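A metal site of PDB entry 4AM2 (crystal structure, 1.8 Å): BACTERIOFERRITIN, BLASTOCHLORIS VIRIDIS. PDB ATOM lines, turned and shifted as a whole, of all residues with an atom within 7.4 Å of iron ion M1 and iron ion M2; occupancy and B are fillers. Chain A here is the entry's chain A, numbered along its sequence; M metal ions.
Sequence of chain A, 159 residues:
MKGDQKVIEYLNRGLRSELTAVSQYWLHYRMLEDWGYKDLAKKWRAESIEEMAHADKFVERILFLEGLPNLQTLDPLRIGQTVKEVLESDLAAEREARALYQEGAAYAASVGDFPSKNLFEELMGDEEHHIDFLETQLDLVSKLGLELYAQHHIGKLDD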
ATOM      1  N   GLY A  14       3.982   8.476 -27.877  1.00  0.00           N
ATOM      2  CA  GLY A  14       4.586   9.647 -27.210  1.00  0.00           C
ATOM      3  C   GLY A  14       3.670  10.863 -27.428  1.00  0.00           C
ATOM      4  O   GLY A  14       3.442  11.665 -26.517  1.00  0.00           O
ATOM      5  N   SER A  17       0.892  10.761 -25.123  1.00  0.00           N
ATOM      6  CA  SER A  17       1.295  11.027 -23.759  1.00  0.00           C
ATOM      7  C   SER A  17       1.438  12.574 -23.591  1.00  0.00           C
ATOM      8  O   SER A  17       0.964  13.132 -22.585  1.00  0.00           O
ATOM      9  CB  SER A  17       2.665  10.285 -23.554  1.00  0.00           C
ATOM     10  OG  SER A  17       3.081  10.574 -22.248  1.00  0.00           O
ATOM     11  N   GLU A  18       2.020  13.270 -24.587  1.00  0.00           N
ATOM     12  CA  GLU A  18       2.210  14.709 -24.512  1.00  0.00           C
ATOM     13  C   GLU A  18       0.860  15.384 -24.596  1.00  0.00           C
ATOM     14  O   GLU A  18       0.667  16.399 -23.909  1.00  0.00           O
ATOM     15  CB  GLU A  18       3.114  15.172 -25.664  1.00  0.00           C
ATOM     16  CG  GLU A  18       4.608  14.776 -25.502  1.00  0.00           C
ATOM     17  CD  GLU A  18       5.210  15.416 -24.235  1.00  0.00           C
ATOM     18  OE1 GLU A  18       4.676  16.400 -23.656  1.00  0.00           O
ATOM     19  OE2 GLU A  18       6.242  14.935 -23.816  1.00  0.00           O
ATOM     20  N   ALA A  21      -0.555  15.264 -21.281  1.00  0.00           N
ATOM     21  CA  ALA A  21       0.111  16.164 -20.294  1.00  0.00           C
ATOM     22  C   ALA A  21      -0.288  17.621 -20.589  1.00  0.00           C
ATOM     23  O   ALA A  21      -0.440  18.449 -19.674  1.00  0.00           O
ATOM     24  CB  ALA A  21       1.627  16.039 -20.384  1.00  0.00           C
ATOM     25  N   TYR A  25      -1.924  19.476 -17.445  1.00  0.00           N
ATOM     26  CA  TYR A  25      -1.263  20.649 -16.900  1.00  0.00           C
ATOM     27  C   TYR A  25      -2.130  21.886 -17.092  1.00  0.00           C
ATOM     28  O   TYR A  25      -2.190  22.748 -16.187  1.00  0.00           O
ATOM     29  CB  TYR A  25       0.109  20.916 -17.556  1.00  0.00           C
ATOM     30  CG  TYR A  25       1.262  20.079 -16.981  1.00  0.00           C
ATOM     31  CD1 TYR A  25       1.561  20.160 -15.612  1.00  0.00           C
ATOM     32  CD2 TYR A  25       2.046  19.273 -17.790  1.00  0.00           C
ATOM     33  CE1 TYR A  25       2.631  19.435 -15.044  1.00  0.00           C
ATOM     34  CE2 TYR A  25       3.137  18.508 -17.257  1.00  0.00           C
ATOM     35  CZ  TYR A  25       3.414  18.611 -15.908  1.00  0.00           C
ATOM     36  OH  TYR A  25       4.450  17.925 -15.311  1.00  0.00           O
ATOM     37  N   GLU A  47       4.517  24.968 -17.732  1.00  0.00           N
ATOM     38  CA  GLU A  47       4.755  23.521 -17.963  1.00  0.00           C
ATOM     39  C   GLU A  47       3.857  23.007 -19.095  1.00  0.00           C
ATOM     40  O   GLU A  47       4.337  22.248 -19.986  1.00  0.00           O
ATOM     41  CB  GLU A  47       4.429  22.679 -16.753  1.00  0.00           C
ATOM     42  CG  GLU A  47       5.385  22.815 -15.569  1.00  0.00           C
ATOM     43  CD  GLU A  47       6.872  22.576 -15.876  1.00  0.00           C
ATOM     44  OE1 GLU A  47       7.296  22.413 -17.055  1.00  0.00           O
ATOM     45  OE2 GLU A  47       7.646  22.563 -14.875  1.00  0.00           O
ATOM     46  N   GLU A  50       5.317  24.095 -22.374  1.00  0.00           N
ATOM     47  CA  GLU A  50       6.474  23.203 -22.670  1.00  0.00           C
ATOM     48  C   GLU A  50       6.039  21.885 -23.291  1.00  0.00           C
ATOM     49  O   GLU A  50       6.704  21.402 -24.198  1.00  0.00           O
ATOM     50  CB  GLU A  50       7.350  22.932 -21.442  1.00  0.00           C
ATOM     51  CG  GLU A  50       8.022  24.219 -21.034  1.00  0.00           C
ATOM     52  CD  GLU A  50       9.023  24.074 -19.904  1.00  0.00           C
ATOM     53  OE1 GLU A  50       9.403  22.901 -19.499  1.00  0.00           O
ATOM     54  OE2 GLU A  50       9.412  25.174 -19.441  1.00  0.00           O
ATOM     55  N   GLU A  51       4.979  21.275 -22.761  1.00  0.00           N
ATOM     56  CA  GLU A  51       4.472  19.989 -23.268  1.00  0.00           C
ATOM     57  C   GLU A  51       3.867  20.210 -24.666  1.00  0.00           C
ATOM     58  O   GLU A  51       3.893  19.255 -25.483  1.00  0.00           O
ATOM     59  CB  GLU A  51       3.423  19.361 -22.321  1.00  0.00           C
ATOM     60  CG  GLU A  51       3.967  19.063 -20.891  1.00  0.00           C
ATOM     61  CD  GLU A  51       4.952  17.888 -20.881  1.00  0.00           C
ATOM     62  OE1 GLU A  51       5.979  17.981 -21.488  1.00  0.00           O
ATOM     63  OE2 GLU A  51       4.746  16.826 -20.218  1.00  0.00           O
ATOM     64  N   MET A  52       3.314  21.422 -24.917  1.00  0.00           N
ATOM     65  CA  MET A  52       2.783  21.664 -26.247  1.00  0.00           C
ATOM     66  C   MET A  52       3.896  21.537 -27.293  1.00  0.00           C
ATOM     67  O   MET A  52       3.660  21.000 -28.369  1.00  0.00           O
ATOM     68  CB  MET A  52       2.075  23.019 -26.403  1.00  0.00           C
ATOM     69  CG  MET A  52       0.791  23.049 -25.478  1.00  0.00           C
ATOM     70  SD  MET A  52       0.221  24.784 -25.423  1.00  0.00           S
ATOM     71  CE  MET A  52      -0.730  24.699 -23.878  1.00  0.00           C
ATOM     72  N   ALA A  53       5.048  22.091 -26.997  1.00  0.00           N
ATOM     73  CA  ALA A  53       6.182  22.048 -27.882  1.00  0.00           C
ATOM     74  C   ALA A  53       6.678  20.615 -28.101  1.00  0.00           C
ATOM     75  O   ALA A  53       7.072  20.271 -29.206  1.00  0.00           O
ATOM     76  CB  ALA A  53       7.266  23.011 -27.370  1.00  0.00           C
ATOM     77  N   HIS A  54       6.644  19.791 -27.050  1.00  0.00           N
ATOM     78  CA  HIS A  54       6.948  18.331 -27.162  1.00  0.00           C
ATOM     79  C   HIS A  54       5.984  17.630 -28.092  1.00  0.00           C
ATOM     80  O   HIS A  54       6.440  16.830 -28.932  1.00  0.00           O
ATOM     81  CB  HIS A  54       6.890  17.643 -25.780  1.00  0.00           C
ATOM     82  CG  HIS A  54       7.977  18.090 -24.844  1.00  0.00           C
ATOM     83  ND1 HIS A  54       8.093  17.624 -23.554  1.00  0.00           N
ATOM     84  CD2 HIS A  54       9.061  18.930 -25.051  1.00  0.00           C
ATOM     85  CE1 HIS A  54       9.188  18.154 -22.987  1.00  0.00           C
ATOM     86  NE2 HIS A  54       9.763  18.984 -23.879  1.00  0.00           N
ATOM     87  N   ALA A  55       4.686  17.969 -27.998  1.00  0.00           N
ATOM     88  CA  ALA A  55       3.629  17.305 -28.847  1.00  0.00           C
ATOM     89  C   ALA A  55       3.967  17.672 -30.299  1.00  0.00           C
ATOM     90  O   ALA A  55       3.942  16.806 -31.165  1.00  0.00           O
ATOM     91  CB  ALA A  55       2.238  17.786 -28.476  1.00  0.00           C
ATOM     92  N   PHE A  58       6.735  15.653 -31.864  1.00  0.00           N
ATOM     93  CA  PHE A  58       6.302  14.332 -32.280  1.00  0.00           C
ATOM     94  C   PHE A  58       5.492  14.392 -33.564  1.00  0.00           C
ATOM     95  O   PHE A  58       5.709  13.556 -34.481  1.00  0.00           O
ATOM     96  CB  PHE A  58       5.471  13.612 -31.191  1.00  0.00           C
ATOM     97  CG  PHE A  58       6.294  13.018 -30.099  1.00  0.00           C
ATOM     98  CD1 PHE A  58       7.333  12.109 -30.398  1.00  0.00           C
ATOM     99  CD2 PHE A  58       5.995  13.317 -28.777  1.00  0.00           C
ATOM    100  CE1 PHE A  58       8.071  11.515 -29.389  1.00  0.00           C
ATOM    101  CE2 PHE A  58       6.669  12.697 -27.752  1.00  0.00           C
ATOM    102  CZ  PHE A  58       7.717  11.783 -28.050  1.00  0.00           C
ATOM    103  N   ASP A  90       0.228  14.809 -11.473  1.00  0.00           N
ATOM    104  CA  ASP A  90       1.219  15.162 -12.507  1.00  0.00           C
ATOM    105  C   ASP A  90       2.471  14.349 -12.403  1.00  0.00           C
ATOM    106  O   ASP A  90       3.055  13.964 -13.408  1.00  0.00           O
ATOM    107  CB  ASP A  90       1.475  16.650 -12.483  1.00  0.00           C
ATOM    108  CG  ASP A  90       0.256  17.437 -13.019  1.00  0.00           C
ATOM    109  OD1 ASP A  90      -0.537  16.891 -13.850  1.00  0.00           O
ATOM    110  OD2 ASP A  90       0.086  18.612 -12.617  1.00  0.00           O
ATOM    111  N   ALA A  93       1.940  10.935 -13.959  1.00  0.00           N
ATOM    112  CA  ALA A  93       1.870  10.974 -15.421  1.00  0.00           C
ATOM    113  C   ALA A  93       3.299  11.141 -15.965  1.00  0.00           C
ATOM    114  O   ALA A  93       3.682  10.514 -16.988  1.00  0.00           O
ATOM    115  CB  ALA A  93       0.953  12.072 -15.971  1.00  0.00           C
ATOM    116  N   GLU A  94       4.114  11.953 -15.293  1.00  0.00           N
ATOM    117  CA  GLU A  94       5.457  12.167 -15.784  1.00  0.00           C
ATOM    118  C   GLU A  94       6.298  10.911 -15.676  1.00  0.00           C
ATOM    119  O   GLU A  94       7.092  10.648 -16.576  1.00  0.00           O
ATOM    120  CB  GLU A  94       6.232  13.267 -15.009  1.00  0.00           C
ATOM    121  CG  GLU A  94       5.624  14.638 -15.324  1.00  0.00           C
ATOM    122  CD  GLU A  94       6.113  15.164 -16.669  1.00  0.00           C
ATOM    123  OE1 GLU A  94       7.040  14.482 -17.292  1.00  0.00           O
ATOM    124  OE2 GLU A  94       5.602  16.243 -17.104  1.00  0.00           O
ATOM    125  N   ALA A  97       5.387   8.821 -18.657  1.00  0.00           N
ATOM    126  CA  ALA A  97       5.982   9.435 -19.894  1.00  0.00           C
ATOM    127  C   ALA A  97       7.511   9.160 -19.975  1.00  0.00           C
ATOM    128  O   ALA A  97       8.037   8.818 -21.042  1.00  0.00           O
ATOM    129  CB  ALA A  97       5.685  10.968 -19.952  1.00  0.00           C
ATOM    130  N   TYR A 101       9.427   7.107 -22.977  1.00  0.00           N
ATOM    131  CA  TYR A 101      10.510   7.616 -23.824  1.00  0.00           C
ATOM    132  C   TYR A 101      11.771   6.798 -23.707  1.00  0.00           C
ATOM    133  O   TYR A 101      12.506   6.670 -24.677  1.00  0.00           O
ATOM    134  CB  TYR A 101      10.814   9.092 -23.498  1.00  0.00           C
ATOM    135  CG  TYR A 101       9.562   9.985 -23.716  1.00  0.00           C
ATOM    136  CD1 TYR A 101       8.488   9.534 -24.497  1.00  0.00           C
ATOM    137  CD2 TYR A 101       9.446  11.234 -23.076  1.00  0.00           C
ATOM    138  CE1 TYR A 101       7.333  10.295 -24.624  1.00  0.00           C
ATOM    139  CE2 TYR A 101       8.293  12.018 -23.197  1.00  0.00           C
ATOM    140  CZ  TYR A 101       7.268  11.570 -23.993  1.00  0.00           C
ATOM    141  OH  TYR A 101       6.156  12.343 -24.144  1.00  0.00           O
ATOM    142  N   LEU A 123      13.637  14.259 -24.867  1.00  0.00           N
ATOM    143  CA  LEU A 123      12.404  14.377 -24.107  1.00  0.00           C
ATOM    144  C   LEU A 123      12.478  13.620 -22.785  1.00  0.00           C
ATOM    145  O   LEU A 123      11.889  14.033 -21.787  1.00  0.00           O
ATOM    146  CB  LEU A 123      11.223  13.891 -24.969  1.00  0.00           C
ATOM    147  CG  LEU A 123      10.854  14.756 -26.156  1.00  0.00           C
ATOM    148  CD1 LEU A 123       9.554  14.203 -26.744  1.00  0.00           C
ATOM    149  CD2 LEU A 123      10.587  16.112 -25.682  1.00  0.00           C
ATOM    150  N   ASP A 126      14.002  16.029 -20.457  1.00  0.00           N
ATOM    151  CA  ASP A 126      13.094  17.067 -20.072  1.00  0.00           C
ATOM    152  C   ASP A 126      12.062  16.573 -19.035  1.00  0.00           C
ATOM    153  O   ASP A 126      11.728  17.300 -18.099  1.00  0.00           O
ATOM    154  CB  ASP A 126      12.307  17.517 -21.290  1.00  0.00           C
ATOM    155  CG  ASP A 126      13.168  18.262 -22.317  1.00  0.00           C
ATOM    156  OD1 ASP A 126      14.270  18.716 -21.919  1.00  0.00           O
ATOM    157  OD2 ASP A 126      12.738  18.453 -23.530  1.00  0.00           O
ATOM    158  N   GLU A 127      11.522  15.393 -19.251  1.00  0.00           N
ATOM    159  CA  GLU A 127      10.571  14.845 -18.287  1.00  0.00           C
ATOM    160  C   GLU A 127      11.222  14.586 -16.926  1.00  0.00           C
ATOM    161  O   GLU A 127      10.563  14.794 -15.881  1.00  0.00           O
ATOM    162  CB  GLU A 127       9.950  13.507 -18.754  1.00  0.00           C
ATOM    163  CG  GLU A 127       9.245  13.550 -20.097  1.00  0.00           C
ATOM    164  CD  GLU A 127       8.279  14.724 -20.278  1.00  0.00           C
ATOM    165  OE1 GLU A 127       7.650  15.170 -19.301  1.00  0.00           O
ATOM    166  OE2 GLU A 127       8.140  15.185 -21.418  1.00  0.00           O
ATOM    167  N   GLU A 128      12.500  14.247 -16.920  1.00  0.00           N
ATOM    168  CA  GLU A 128      13.179  14.110 -15.625  1.00  0.00           C
ATOM    169  C   GLU A 128      13.282  15.459 -14.880  1.00  0.00           C
ATOM    170  O   GLU A 128      13.150  15.447 -13.673  1.00  0.00           O
ATOM    171  CB  GLU A 128      14.556  13.393 -15.781  1.00  0.00           C
ATOM    172  CG  GLU A 128      14.283  11.863 -15.902  1.00  0.00           C
ATOM    173  CD  GLU A 128      15.554  11.010 -15.891  1.00  0.00           C
ATOM    174  OE1 GLU A 128      16.673  11.537 -15.742  1.00  0.00           O
ATOM    175  OE2 GLU A 128      15.474   9.732 -16.085  1.00  0.00           O
ATOM    176  N   HIS A 129      13.435  16.570 -15.584  1.00  0.00           N
ATOM    177  CA  HIS A 129      13.417  17.882 -14.955  1.00  0.00           C
ATOM    178  C   HIS A 129      12.016  18.151 -14.362  1.00  0.00           C
ATOM    179  O   HIS A 129      11.942  18.644 -13.226  1.00  0.00           O
ATOM    180  CB  HIS A 129      13.787  18.989 -15.914  1.00  0.00           C
ATOM    181  CG  HIS A 129      15.228  19.037 -16.287  1.00  0.00           C
ATOM    182  ND1 HIS A 129      16.236  19.133 -15.344  1.00  0.00           N
ATOM    183  CD2 HIS A 129      15.874  19.040 -17.553  1.00  0.00           C
ATOM    184  CE1 HIS A 129      17.445  19.160 -15.985  1.00  0.00           C
ATOM    185  NE2 HIS A 129      17.224  19.089 -17.321  1.00  0.00           N
ATOM    186  N   HIS A 130      10.958  17.817 -15.095  1.00  0.00           N
ATOM    187  CA  HIS A 130       9.598  17.874 -14.556  1.00  0.00           C
ATOM    188  C   HIS A 130       9.436  17.046 -13.310  1.00  0.00           C
ATOM    189  O   HIS A 130       8.793  17.508 -12.354  1.00  0.00           O
ATOM    190  CB  HIS A 130       8.485  17.540 -15.592  1.00  0.00           C
ATOM    191  CG  HIS A 130       8.480  18.458 -16.791  1.00  0.00           C
ATOM    192  ND1 HIS A 130       7.785  18.209 -17.926  1.00  0.00           N
ATOM    193  CD2 HIS A 130       9.188  19.660 -17.041  1.00  0.00           C
ATOM    194  CE1 HIS A 130       7.988  19.181 -18.829  1.00  0.00           C
ATOM    195  NE2 HIS A 130       8.847  20.069 -18.322  1.00  0.00           N
ATOM    196  N   ILE A 131       9.925  15.799 -13.325  1.00  0.00           N
ATOM    197  CA  ILE A 131       9.829  14.892 -12.179  1.00  0.00           C
ATOM    198  C   ILE A 131      10.569  15.509 -10.958  1.00  0.00           C
ATOM    199  O   ILE A 131      10.074  15.524  -9.825  1.00  0.00           O
ATOM    200  CB  ILE A 131      10.410  13.525 -12.564  1.00  0.00           C
ATOM    201  CG1 ILE A 131       9.389  12.769 -13.442  1.00  0.00           C
ATOM    202  CG2 ILE A 131      10.679  12.667 -11.310  1.00  0.00           C
ATOM    203  CD1 ILE A 131      10.068  11.567 -14.072  1.00  0.00           C
ATOM    204  N   LEU A 134       8.445  18.305  -9.508  1.00  0.00           N
ATOM    205  CA  LEU A 134       7.254  17.818  -8.792  1.00  0.00           C
ATOM    206  C   LEU A 134       7.643  17.128  -7.494  1.00  0.00           C
ATOM    207  O   LEU A 134       6.980  17.330  -6.442  1.00  0.00           O
ATOM    208  CB  LEU A 134       6.453  16.848  -9.667  1.00  0.00           C
ATOM    209  CG  LEU A 134       5.829  17.555 -10.872  1.00  0.00           C
ATOM    210  CD1 LEU A 134       5.392  16.493 -11.893  1.00  0.00           C
ATOM    211  CD2 LEU A 134       4.694  18.531 -10.430  1.00  0.00           C
HETATM  212 FE    FE M   1       6.879  16.433 -22.510  1.00  0.00          FE
HETATM  213 FE    FE M   2       6.638  16.871 -18.567  1.00  0.00          FE
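Within 4 Å of iron ion M1: Glu 18, Glu 51, His 54 and Glu 127. The nearest printed residue that does not touch iron ion M1 is Tyr 101 (4.5 Å).
ND1 of His 54 binds iron ion M1. Iron ion M1 is bound by OE1 of Glu 51 (2.1 Å). The side-chain carboxylate (OE2) of Glu 127 binds iron ion M1. The side-chain carboxylate (OE2) of Glu 18 is bound to iron ion M1, 2.1 Å away. OE1 of Glu 18 binds iron ion M1. Iron ion M1 has five donor atoms within binding distance.
Iron ion M2 is bound by ND1 of His 130 (1.9 Å), OE2 of Glu 94 (1.9 Å), OE1 of Glu 127 (2.1 Å) and OE2 of Glu 51 (2.5 Å). Slightly farther from iron ion M2 lies OE1 of Glu 94 (2.7 Å).
OH of Tyr 25 sits close to OE2 of Glu 94 (2.7 Å). OE1 of Glu 47 sits at hydrogen-bond distance from NE2 of His 130, 3.1 Å away. NE2 of His 54 sits at hydrogen-bond distance from OD2 of Asp 126 (3.0 Å). The side-chain carboxylate of Glu 18 sits close to the side-chain hydroxyl of Tyr 101, 2.6 Å away. A ring nitrogen (NE2) of His 130 sits at hydrogen-bond distance from the side-chain carboxylate of Glu 50, at 3.1 Å.
Four residues have an atom within 4 Å of iron ion M2: Glu 51, Glu 94, Glu 127 and His 130. Along chain A the residues within 4 Å of iron ion M2 span positions 51 to 130.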
